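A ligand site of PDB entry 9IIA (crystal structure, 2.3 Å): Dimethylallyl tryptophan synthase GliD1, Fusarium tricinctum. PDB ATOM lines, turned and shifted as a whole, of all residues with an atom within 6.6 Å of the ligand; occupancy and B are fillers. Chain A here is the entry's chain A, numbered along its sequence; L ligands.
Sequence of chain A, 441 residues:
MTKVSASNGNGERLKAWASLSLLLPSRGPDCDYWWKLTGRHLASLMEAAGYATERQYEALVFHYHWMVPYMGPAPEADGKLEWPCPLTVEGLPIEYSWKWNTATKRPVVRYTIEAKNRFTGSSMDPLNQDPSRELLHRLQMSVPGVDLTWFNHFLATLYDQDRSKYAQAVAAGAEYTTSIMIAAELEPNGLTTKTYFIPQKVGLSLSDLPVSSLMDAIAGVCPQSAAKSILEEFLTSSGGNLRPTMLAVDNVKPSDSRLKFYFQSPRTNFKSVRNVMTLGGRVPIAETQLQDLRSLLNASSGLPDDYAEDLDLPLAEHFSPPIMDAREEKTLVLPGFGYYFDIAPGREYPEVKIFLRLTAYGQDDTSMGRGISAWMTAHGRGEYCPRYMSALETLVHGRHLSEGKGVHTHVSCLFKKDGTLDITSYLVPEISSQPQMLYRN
Merely in contact with the ligand: Phe 355.
Hydrophobic or aromatic side chains within 4 Å of the ligand: Tyr 196, Tyr 262, Tyr 340, Phe 355 and Tyr 426.
Of the 23 residues printed, 10 come within 4 Å of the ligand.
The nearest printed residue that does not touch the ligand is Glu 185 (4.04 Å).
The backbone carbonyl oxygen (O) of Lys 260 lies within hydrogen-bond range of the backbone NH (N) of Ala 248 (2.8 Å).
The backbone NH of Tyr 262 sits at hydrogen-bond distance from the backbone carbonyl oxygen of Met 246, 2.8 Å away.
The backbone NH (N) of Tyr 340 lies within hydrogen-bond range of the backbone carbonyl oxygen (O) of Lys 353 (2.9 Å).
NZ of Lys 194 is in salt-bridge range of OE2 of Glu 185 (2.9 Å).
NH1 of Arg 110 is in salt-bridge range of OE2 of Glu 185.
The backbone NH (N) of Ser 97 is in hydrogen-bond range of the backbone carbonyl oxygen (O) of Arg 110, 2.7 Å away.
The side-chain carboxylate (OE2) of Glu 187 lies within salt-bridge range of the guanidinium group (NH1) of Arg 110 (3.3 Å).
The guanidinium group (NH2) of Arg 258 lies within salt-bridge range of the side-chain carboxylate (OE2) of Glu 185, 3.5 Å away.
O1 of the ligand lies within hydrogen-bond range of OH of Tyr 426, at 2.5 Å.
The side-chain amino group of Lys 260 is in salt-bridge range of an oxygen (O7) of the ligand (2.5 Å).
The side-chain hydroxyl (OH) of Tyr 262 sits at hydrogen-bond distance from an oxygen (O2) of the ligand.
O5 of the ligand lies within salt-bridge range of NZ of Lys 353 (2.6 Å).
An oxygen (O3) of the ligand is in hydrogen-bond range of the side-chain hydroxyl of Tyr 196 (2.7 Å).
NZ of Lys 194 is in salt-bridge range of O7 of the ligand, 2.7 Å away.
The guanidinium group (NH2) of Arg 110 is in salt-bridge range of an oxygen (O6) of the ligand.
The side-chain hydroxyl (OH) of Tyr 340 sits at hydrogen-bond distance from an oxygen (O5) of the ligand (3.3 Å).
NH1 of Arg 258 lies within salt-bridge range of O7 of the ligand.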
ATOM      1  N   GLU A  95      -8.320  16.856   5.107  1.00  0.00           N
ATOM      2  CA  GLU A  95      -8.688  18.083   5.783  1.00  0.00           C
ATOM      3  C   GLU A  95      -7.563  18.435   6.730  1.00  0.00           C
ATOM      4  O   GLU A  95      -7.072  17.558   7.454  1.00  0.00           O
ATOM      5  CB  GLU A  95     -10.016  17.935   6.550  1.00  0.00           C
ATOM      6  CG  GLU A  95     -10.353  19.091   7.530  1.00  0.00           C
ATOM      7  CD  GLU A  95     -11.639  18.806   8.322  1.00  0.00           C
ATOM      8  OE1 GLU A  95     -11.553  18.005   9.291  1.00  0.00           O
ATOM      9  OE2 GLU A  95     -12.706  19.387   7.989  1.00  0.00           O
ATOM     10  N   SER A  97      -6.043  20.877   9.946  1.00  0.00           N
ATOM     11  CA  SER A  97      -6.511  21.703  11.040  1.00  0.00           C
ATOM     12  C   SER A  97      -5.361  22.539  11.580  1.00  0.00           C
ATOM     13  O   SER A  97      -4.190  22.114  11.589  1.00  0.00           O
ATOM     14  CB  SER A  97      -7.113  20.862  12.167  1.00  0.00           C
ATOM     15  OG  SER A  97      -6.122  20.054  12.761  1.00  0.00           O
ATOM     16  N   LYS A  99      -4.569  24.254  15.086  1.00  0.00           N
ATOM     17  CA  LYS A  99      -4.862  24.551  16.478  1.00  0.00           C
ATOM     18  C   LYS A  99      -4.158  25.834  16.858  1.00  0.00           C
ATOM     19  O   LYS A  99      -2.949  25.978  16.689  1.00  0.00           O
ATOM     20  CB  LYS A  99      -4.433  23.434  17.400  1.00  0.00           C
ATOM     21  CG  LYS A  99      -5.144  23.501  18.740  1.00  0.00           C
ATOM     22  CD  LYS A  99      -4.267  22.974  19.844  1.00  0.00           C
ATOM     23  CE  LYS A  99      -4.807  21.653  20.363  1.00  0.00           C
ATOM     24  NZ  LYS A  99      -4.514  21.483  21.821  1.00  0.00           N
ATOM     25  N   ARG A 110      -2.259  19.793  12.042  1.00  0.00           N
ATOM     26  CA  ARG A 110      -2.596  18.389  11.856  1.00  0.00           C
ATOM     27  C   ARG A 110      -3.490  18.243  10.630  1.00  0.00           C
ATOM     28  O   ARG A 110      -3.902  19.236  10.010  1.00  0.00           O
ATOM     29  CB  ARG A 110      -3.238  17.810  13.129  1.00  0.00           C
ATOM     30  CG  ARG A 110      -2.329  17.949  14.361  1.00  0.00           C
ATOM     31  CD  ARG A 110      -3.099  18.104  15.649  1.00  0.00           C
ATOM     32  NE  ARG A 110      -4.435  18.670  15.406  1.00  0.00           N
ATOM     33  CZ  ARG A 110      -5.400  18.729  16.316  1.00  0.00           C
ATOM     34  NH1 ARG A 110      -5.185  18.358  17.571  1.00  0.00           N
ATOM     35  NH2 ARG A 110      -6.611  19.145  15.947  1.00  0.00           N
ATOM     36  N   THR A 112      -6.284  15.117   8.471  1.00  0.00           N
ATOM     37  CA  THR A 112      -7.024  13.857   8.402  1.00  0.00           C
ATOM     38  C   THR A 112      -7.155  13.424   6.945  1.00  0.00           C
ATOM     39  O   THR A 112      -7.364  14.262   6.071  1.00  0.00           O
ATOM     40  CB  THR A 112      -8.409  14.030   9.025  1.00  0.00           C
ATOM     41  OG1 THR A 112      -8.224  14.451  10.389  1.00  0.00           O
ATOM     42  CG2 THR A 112      -9.178  12.737   9.011  1.00  0.00           C
ATOM     43  N   GLU A 185      -1.168  13.205  14.237  1.00  0.00           N
ATOM     44  CA  GLU A 185      -0.994  14.476  14.916  1.00  0.00           C
ATOM     45  C   GLU A 185       0.485  14.837  14.881  1.00  0.00           C
ATOM     46  O   GLU A 185       1.335  14.018  15.242  1.00  0.00           O
ATOM     47  CB  GLU A 185      -1.504  14.400  16.366  1.00  0.00           C
ATOM     48  CG  GLU A 185      -3.025  14.473  16.497  1.00  0.00           C
ATOM     49  CD  GLU A 185      -3.459  14.532  17.951  1.00  0.00           C
ATOM     50  OE1 GLU A 185      -2.577  14.378  18.818  1.00  0.00           O
ATOM     51  OE2 GLU A 185      -4.669  14.716  18.226  1.00  0.00           O
ATOM     52  N   GLU A 187       2.104  16.842  16.734  1.00  0.00           N
ATOM     53  CA  GLU A 187       2.297  17.599  17.961  1.00  0.00           C
ATOM     54  C   GLU A 187       3.746  17.570  18.452  1.00  0.00           C
ATOM     55  O   GLU A 187       4.512  16.699  18.067  1.00  0.00           O
ATOM     56  CB  GLU A 187       1.361  17.024  19.028  1.00  0.00           C
ATOM     57  CG  GLU A 187       0.027  16.560  18.478  1.00  0.00           C
ATOM     58  CD  GLU A 187      -1.136  17.364  19.024  1.00  0.00           C
ATOM     59  OE1 GLU A 187      -0.941  18.093  20.017  1.00  0.00           O
ATOM     60  OE2 GLU A 187      -2.247  17.269  18.465  1.00  0.00           O
ATOM     61  N   LYS A 194      -5.115   8.752  15.284  1.00  0.00           N
ATOM     62  CA  LYS A 194      -6.511   8.707  15.671  1.00  0.00           C
ATOM     63  C   LYS A 194      -7.302   8.105  14.523  1.00  0.00           C
ATOM     64  O   LYS A 194      -6.889   8.173  13.363  1.00  0.00           O
ATOM     65  CB  LYS A 194      -7.056  10.120  15.995  1.00  0.00           C
ATOM     66  CG  LYS A 194      -6.052  10.986  16.743  1.00  0.00           C
ATOM     67  CD  LYS A 194      -6.676  12.291  17.219  1.00  0.00           C
ATOM     68  CE  LYS A 194      -6.815  13.314  16.102  1.00  0.00           C
ATOM     69  NZ  LYS A 194      -7.045  14.705  16.641  1.00  0.00           N
ATOM     70  N   TYR A 196     -11.439   7.830  13.042  1.00  0.00           N
ATOM     71  CA  TYR A 196     -12.825   8.271  13.078  1.00  0.00           C
ATOM     72  C   TYR A 196     -13.682   7.208  12.413  1.00  0.00           C
ATOM     73  O   TYR A 196     -13.330   6.703  11.350  1.00  0.00           O
ATOM     74  CB  TYR A 196     -13.006   9.601  12.342  1.00  0.00           C
ATOM     75  CG  TYR A 196     -12.119  10.684  12.890  1.00  0.00           C
ATOM     76  CD1 TYR A 196     -10.829  10.850  12.417  1.00  0.00           C
ATOM     77  CD2 TYR A 196     -12.575  11.534  13.898  1.00  0.00           C
ATOM     78  CE1 TYR A 196     -10.014  11.823  12.919  1.00  0.00           C
ATOM     79  CE2 TYR A 196     -11.764  12.517  14.421  1.00  0.00           C
ATOM     80  CZ  TYR A 196     -10.470  12.655  13.926  1.00  0.00           C
ATOM     81  OH  TYR A 196      -9.627  13.628  14.424  1.00  0.00           O
ATOM     82  N   MET A 246     -20.762  10.162  14.722  1.00  0.00           N
ATOM     83  CA  MET A 246     -19.380   9.700  14.590  1.00  0.00           C
ATOM     84  C   MET A 246     -18.847   9.303  15.953  1.00  0.00           C
ATOM     85  O   MET A 246     -19.302   9.785  16.991  1.00  0.00           O
ATOM     86  CB  MET A 246     -18.469  10.799  13.995  1.00  0.00           C
ATOM     87  CG  MET A 246     -17.253  10.321  13.208  1.00  0.00           C
ATOM     88  SD  MET A 246     -16.434  11.603  12.198  1.00  0.00           S
ATOM     89  CE  MET A 246     -16.358  13.017  13.308  1.00  0.00           C
ATOM     90  N   ALA A 248     -14.691   8.650  17.645  1.00  0.00           N
ATOM     91  CA  ALA A 248     -13.244   8.663  17.410  1.00  0.00           C
ATOM     92  C   ALA A 248     -12.519   8.116  18.616  1.00  0.00           C
ATOM     93  O   ALA A 248     -12.965   8.259  19.761  1.00  0.00           O
ATOM     94  CB  ALA A 248     -12.684  10.064  17.115  1.00  0.00           C
ATOM     95  N   ASP A 250      -8.155   7.391  19.954  1.00  0.00           N
ATOM     96  CA  ASP A 250      -6.731   7.460  19.689  1.00  0.00           C
ATOM     97  C   ASP A 250      -6.199   6.042  19.638  1.00  0.00           C
ATOM     98  O   ASP A 250      -6.572   5.201  20.456  1.00  0.00           O
ATOM     99  CB  ASP A 250      -6.004   8.255  20.783  1.00  0.00           C
ATOM    100  CG  ASP A 250      -6.665   9.596  21.043  1.00  0.00           C
ATOM    101  OD1 ASP A 250      -6.875  10.339  20.062  1.00  0.00           O
ATOM    102  OD2 ASP A 250      -7.004   9.890  22.214  1.00  0.00           O
ATOM    103  N   ARG A 258      -8.562   8.858  24.393  1.00  0.00           N
ATOM    104  CA  ARG A 258      -9.852   9.513  24.470  1.00  0.00           C
ATOM    105  C   ARG A 258     -10.913   8.657  23.775  1.00  0.00           C
ATOM    106  O   ARG A 258     -10.609   7.711  23.026  1.00  0.00           O
ATOM    107  CB  ARG A 258      -9.789  10.911  23.862  1.00  0.00           C
ATOM    108  CG  ARG A 258      -8.855  11.877  24.609  1.00  0.00           C
ATOM    109  CD  ARG A 258      -8.540  13.107  23.744  1.00  0.00           C
ATOM    110  NE  ARG A 258      -7.885  12.703  22.505  1.00  0.00           N
ATOM    111  CZ  ARG A 258      -7.355  13.533  21.624  1.00  0.00           C
ATOM    112  NH1 ARG A 258      -7.370  14.840  21.811  1.00  0.00           N
ATOM    113  NH2 ARG A 258      -6.764  13.038  20.536  1.00  0.00           N
ATOM    114  N   LYS A 260     -14.332   9.680  21.844  1.00  0.00           N
ATOM    115  CA  LYS A 260     -15.051  10.871  21.419  1.00  0.00           C
ATOM    116  C   LYS A 260     -16.328  10.470  20.720  1.00  0.00           C
ATOM    117  O   LYS A 260     -16.295   9.726  19.733  1.00  0.00           O
ATOM    118  CB  LYS A 260     -14.170  11.708  20.500  1.00  0.00           C
ATOM    119  CG  LYS A 260     -13.248  12.638  21.270  1.00  0.00           C
ATOM    120  CD  LYS A 260     -11.796  12.510  20.850  1.00  0.00           C
ATOM    121  CE  LYS A 260     -11.583  13.195  19.533  1.00  0.00           C
ATOM    122  NZ  LYS A 260     -10.166  13.567  19.316  1.00  0.00           N
ATOM    123  N   TYR A 262     -19.518  11.892  18.831  1.00  0.00           N
ATOM    124  CA  TYR A 262     -19.930  13.080  18.100  1.00  0.00           C
ATOM    125  C   TYR A 262     -21.428  13.112  17.866  1.00  0.00           C
ATOM    126  O   TYR A 262     -22.069  12.072  17.608  1.00  0.00           O
ATOM    127  CB  TYR A 262     -19.241  13.184  16.723  1.00  0.00           C
ATOM    128  CG  TYR A 262     -17.755  13.410  16.782  1.00  0.00           C
ATOM    129  CD1 TYR A 262     -16.889  12.382  17.136  1.00  0.00           C
ATOM    130  CD2 TYR A 262     -17.206  14.661  16.479  1.00  0.00           C
ATOM    131  CE1 TYR A 262     -15.517  12.576  17.205  1.00  0.00           C
ATOM    132  CE2 TYR A 262     -15.819  14.866  16.556  1.00  0.00           C
ATOM    133  CZ  TYR A 262     -14.997  13.804  16.911  1.00  0.00           C
ATOM    134  OH  TYR A 262     -13.646  13.929  16.989  1.00  0.00           O
ATOM    135  N   TYR A 340     -18.619  17.002  20.105  1.00  0.00           N
ATOM    136  CA  TYR A 340     -18.288  15.688  20.645  1.00  0.00           C
ATOM    137  C   TYR A 340     -18.260  15.725  22.170  1.00  0.00           C
ATOM    138  O   TYR A 340     -18.000  16.761  22.787  1.00  0.00           O
ATOM    139  CB  TYR A 340     -16.958  15.119  20.073  1.00  0.00           C
ATOM    140  CG  TYR A 340     -15.604  15.624  20.603  1.00  0.00           C
ATOM    141  CD1 TYR A 340     -15.312  15.601  21.962  1.00  0.00           C
ATOM    142  CD2 TYR A 340     -14.576  15.989  19.719  1.00  0.00           C
ATOM    143  CE1 TYR A 340     -14.065  16.003  22.454  1.00  0.00           C
ATOM    144  CE2 TYR A 340     -13.309  16.391  20.196  1.00  0.00           C
ATOM    145  CZ  TYR A 340     -13.070  16.398  21.572  1.00  0.00           C
ATOM    146  OH  TYR A 340     -11.843  16.776  22.085  1.00  0.00           O
ATOM    147  N   LYS A 353     -16.422  19.439  23.009  1.00  0.00           N
ATOM    148  CA  LYS A 353     -15.938  20.336  21.965  1.00  0.00           C
ATOM    149  C   LYS A 353     -17.090  20.689  21.053  1.00  0.00           C
ATOM    150  O   LYS A 353     -17.838  19.794  20.626  1.00  0.00           O
ATOM    151  CB  LYS A 353     -14.808  19.701  21.145  1.00  0.00           C
ATOM    152  CG  LYS A 353     -14.301  20.631  20.036  1.00  0.00           C
ATOM    153  CD  LYS A 353     -13.073  20.091  19.365  1.00  0.00           C
ATOM    154  CE  LYS A 353     -12.017  19.726  20.381  1.00  0.00           C
ATOM    155  NZ  LYS A 353     -10.692  19.481  19.742  1.00  0.00           N
ATOM    156  N   PHE A 355     -18.300  22.525  17.410  1.00  0.00           N
ATOM    157  CA  PHE A 355     -17.825  22.781  16.049  1.00  0.00           C
ATOM    158  C   PHE A 355     -18.823  23.702  15.367  1.00  0.00           C
ATOM    159  O   PHE A 355     -19.968  23.303  15.144  1.00  0.00           O
ATOM    160  CB  PHE A 355     -17.707  21.468  15.256  1.00  0.00           C
ATOM    161  CG  PHE A 355     -16.771  20.470  15.852  1.00  0.00           C
ATOM    162  CD1 PHE A 355     -15.414  20.502  15.563  1.00  0.00           C
ATOM    163  CD2 PHE A 355     -17.241  19.482  16.726  1.00  0.00           C
ATOM    164  CE1 PHE A 355     -14.537  19.579  16.122  1.00  0.00           C
ATOM    165  CE2 PHE A 355     -16.380  18.555  17.270  1.00  0.00           C
ATOM    166  CZ  PHE A 355     -15.025  18.600  16.965  1.00  0.00           C
ATOM    167  N   SER A 412     -13.592  25.282  16.070  1.00  0.00           N
ATOM    168  CA  SER A 412     -14.001  24.529  17.241  1.00  0.00           C
ATOM    169  C   SER A 412     -13.445  25.141  18.510  1.00  0.00           C
ATOM    170  O   SER A 412     -12.410  25.805  18.508  1.00  0.00           O
ATOM    171  CB  SER A 412     -13.548  23.078  17.129  1.00  0.00           C
ATOM    172  OG  SER A 412     -12.152  23.022  17.339  1.00  0.00           O
ATOM    173  N   LEU A 414     -12.979  24.041  22.841  1.00  0.00           N
ATOM    174  CA  LEU A 414     -13.112  23.160  23.972  1.00  0.00           C
ATOM    175  C   LEU A 414     -12.511  23.869  25.174  1.00  0.00           C
ATOM    176  O   LEU A 414     -11.431  24.441  25.077  1.00  0.00           O
ATOM    177  CB  LEU A 414     -12.424  21.800  23.706  1.00  0.00           C
ATOM    178  CG  LEU A 414     -12.326  20.754  24.835  1.00  0.00           C
ATOM    179  CD1 LEU A 414     -12.420  19.343  24.267  1.00  0.00           C
ATOM    180  CD2 LEU A 414     -11.039  20.904  25.622  1.00  0.00           C
ATOM    181  N   ASP A 422      -9.310  26.160  24.020  1.00  0.00           N
ATOM    182  CA  ASP A 422      -8.616  25.493  22.936  1.00  0.00           C
ATOM    183  C   ASP A 422      -9.422  25.672  21.662  1.00  0.00           C
ATOM    184  O   ASP A 422     -10.554  25.192  21.579  1.00  0.00           O
ATOM    185  CB  ASP A 422      -8.452  24.002  23.235  1.00  0.00           C
ATOM    186  CG  ASP A 422      -7.025  23.530  23.130  1.00  0.00           C
ATOM    187  OD1 ASP A 422      -6.087  24.374  23.104  1.00  0.00           O
ATOM    188  OD2 ASP A 422      -6.837  22.300  23.071  1.00  0.00           O
ATOM    189  N   THR A 424      -9.599  25.668  17.316  1.00  0.00           N
ATOM    190  CA  THR A 424      -9.037  25.037  16.130  1.00  0.00           C
ATOM    191  C   THR A 424      -9.783  25.473  14.884  1.00  0.00           C
ATOM    192  O   THR A 424     -11.018  25.456  14.848  1.00  0.00           O
ATOM    193  CB  THR A 424      -9.098  23.515  16.266  1.00  0.00           C
ATOM    194  OG1 THR A 424      -8.420  23.138  17.462  1.00  0.00           O
ATOM    195  CG2 THR A 424      -8.447  22.831  15.053  1.00  0.00           C
ATOM    196  N   TYR A 426     -10.402  24.299  11.072  1.00  0.00           N
ATOM    197  CA  TYR A 426     -10.326  23.157  10.179  1.00  0.00           C
ATOM    198  C   TYR A 426     -10.415  23.642   8.746  1.00  0.00           C
ATOM    199  O   TYR A 426     -11.379  24.317   8.365  1.00  0.00           O
ATOM    200  CB  TYR A 426     -11.432  22.148  10.460  1.00  0.00           C
ATOM    201  CG  TYR A 426     -11.296  21.462  11.784  1.00  0.00           C
ATOM    202  CD1 TYR A 426     -11.710  22.087  12.966  1.00  0.00           C
ATOM    203  CD2 TYR A 426     -10.760  20.178  11.859  1.00  0.00           C
ATOM    204  CE1 TYR A 426     -11.591  21.456  14.194  1.00  0.00           C
ATOM    205  CE2 TYR A 426     -10.620  19.534  13.087  1.00  0.00           C
ATOM    206  CZ  TYR A 426     -11.043  20.174  14.243  1.00  0.00           C
ATOM    207  OH  TYR A 426     -10.917  19.554  15.466  1.00  0.00           O
HETATM  208  O1  LIG L   1     -10.413  17.103  15.659  1.00  0.00           O
HETATM  209  P1  LIG L   1     -11.083  16.254  16.694  1.00  0.00           P
HETATM  210  O2  LIG L   1     -12.559  16.262  16.476  1.00  0.00           O
HETATM  211  O3  LIG L   1     -10.547  14.863  16.600  1.00  0.00           O
HETATM  212  O4  LIG L   1     -10.731  16.839  18.181  1.00  0.00           O
HETATM  213  P2  LIG L   1      -9.206  16.841  18.770  1.00  0.00           P
HETATM  214  O5  LIG L   1      -9.219  17.333  20.198  1.00  0.00           O
HETATM  215  O6  LIG L   1      -8.350  17.753  17.930  1.00  0.00           O
HETATM  216  O7  LIG L   1      -8.609  15.461  18.719  1.00  0.00           O
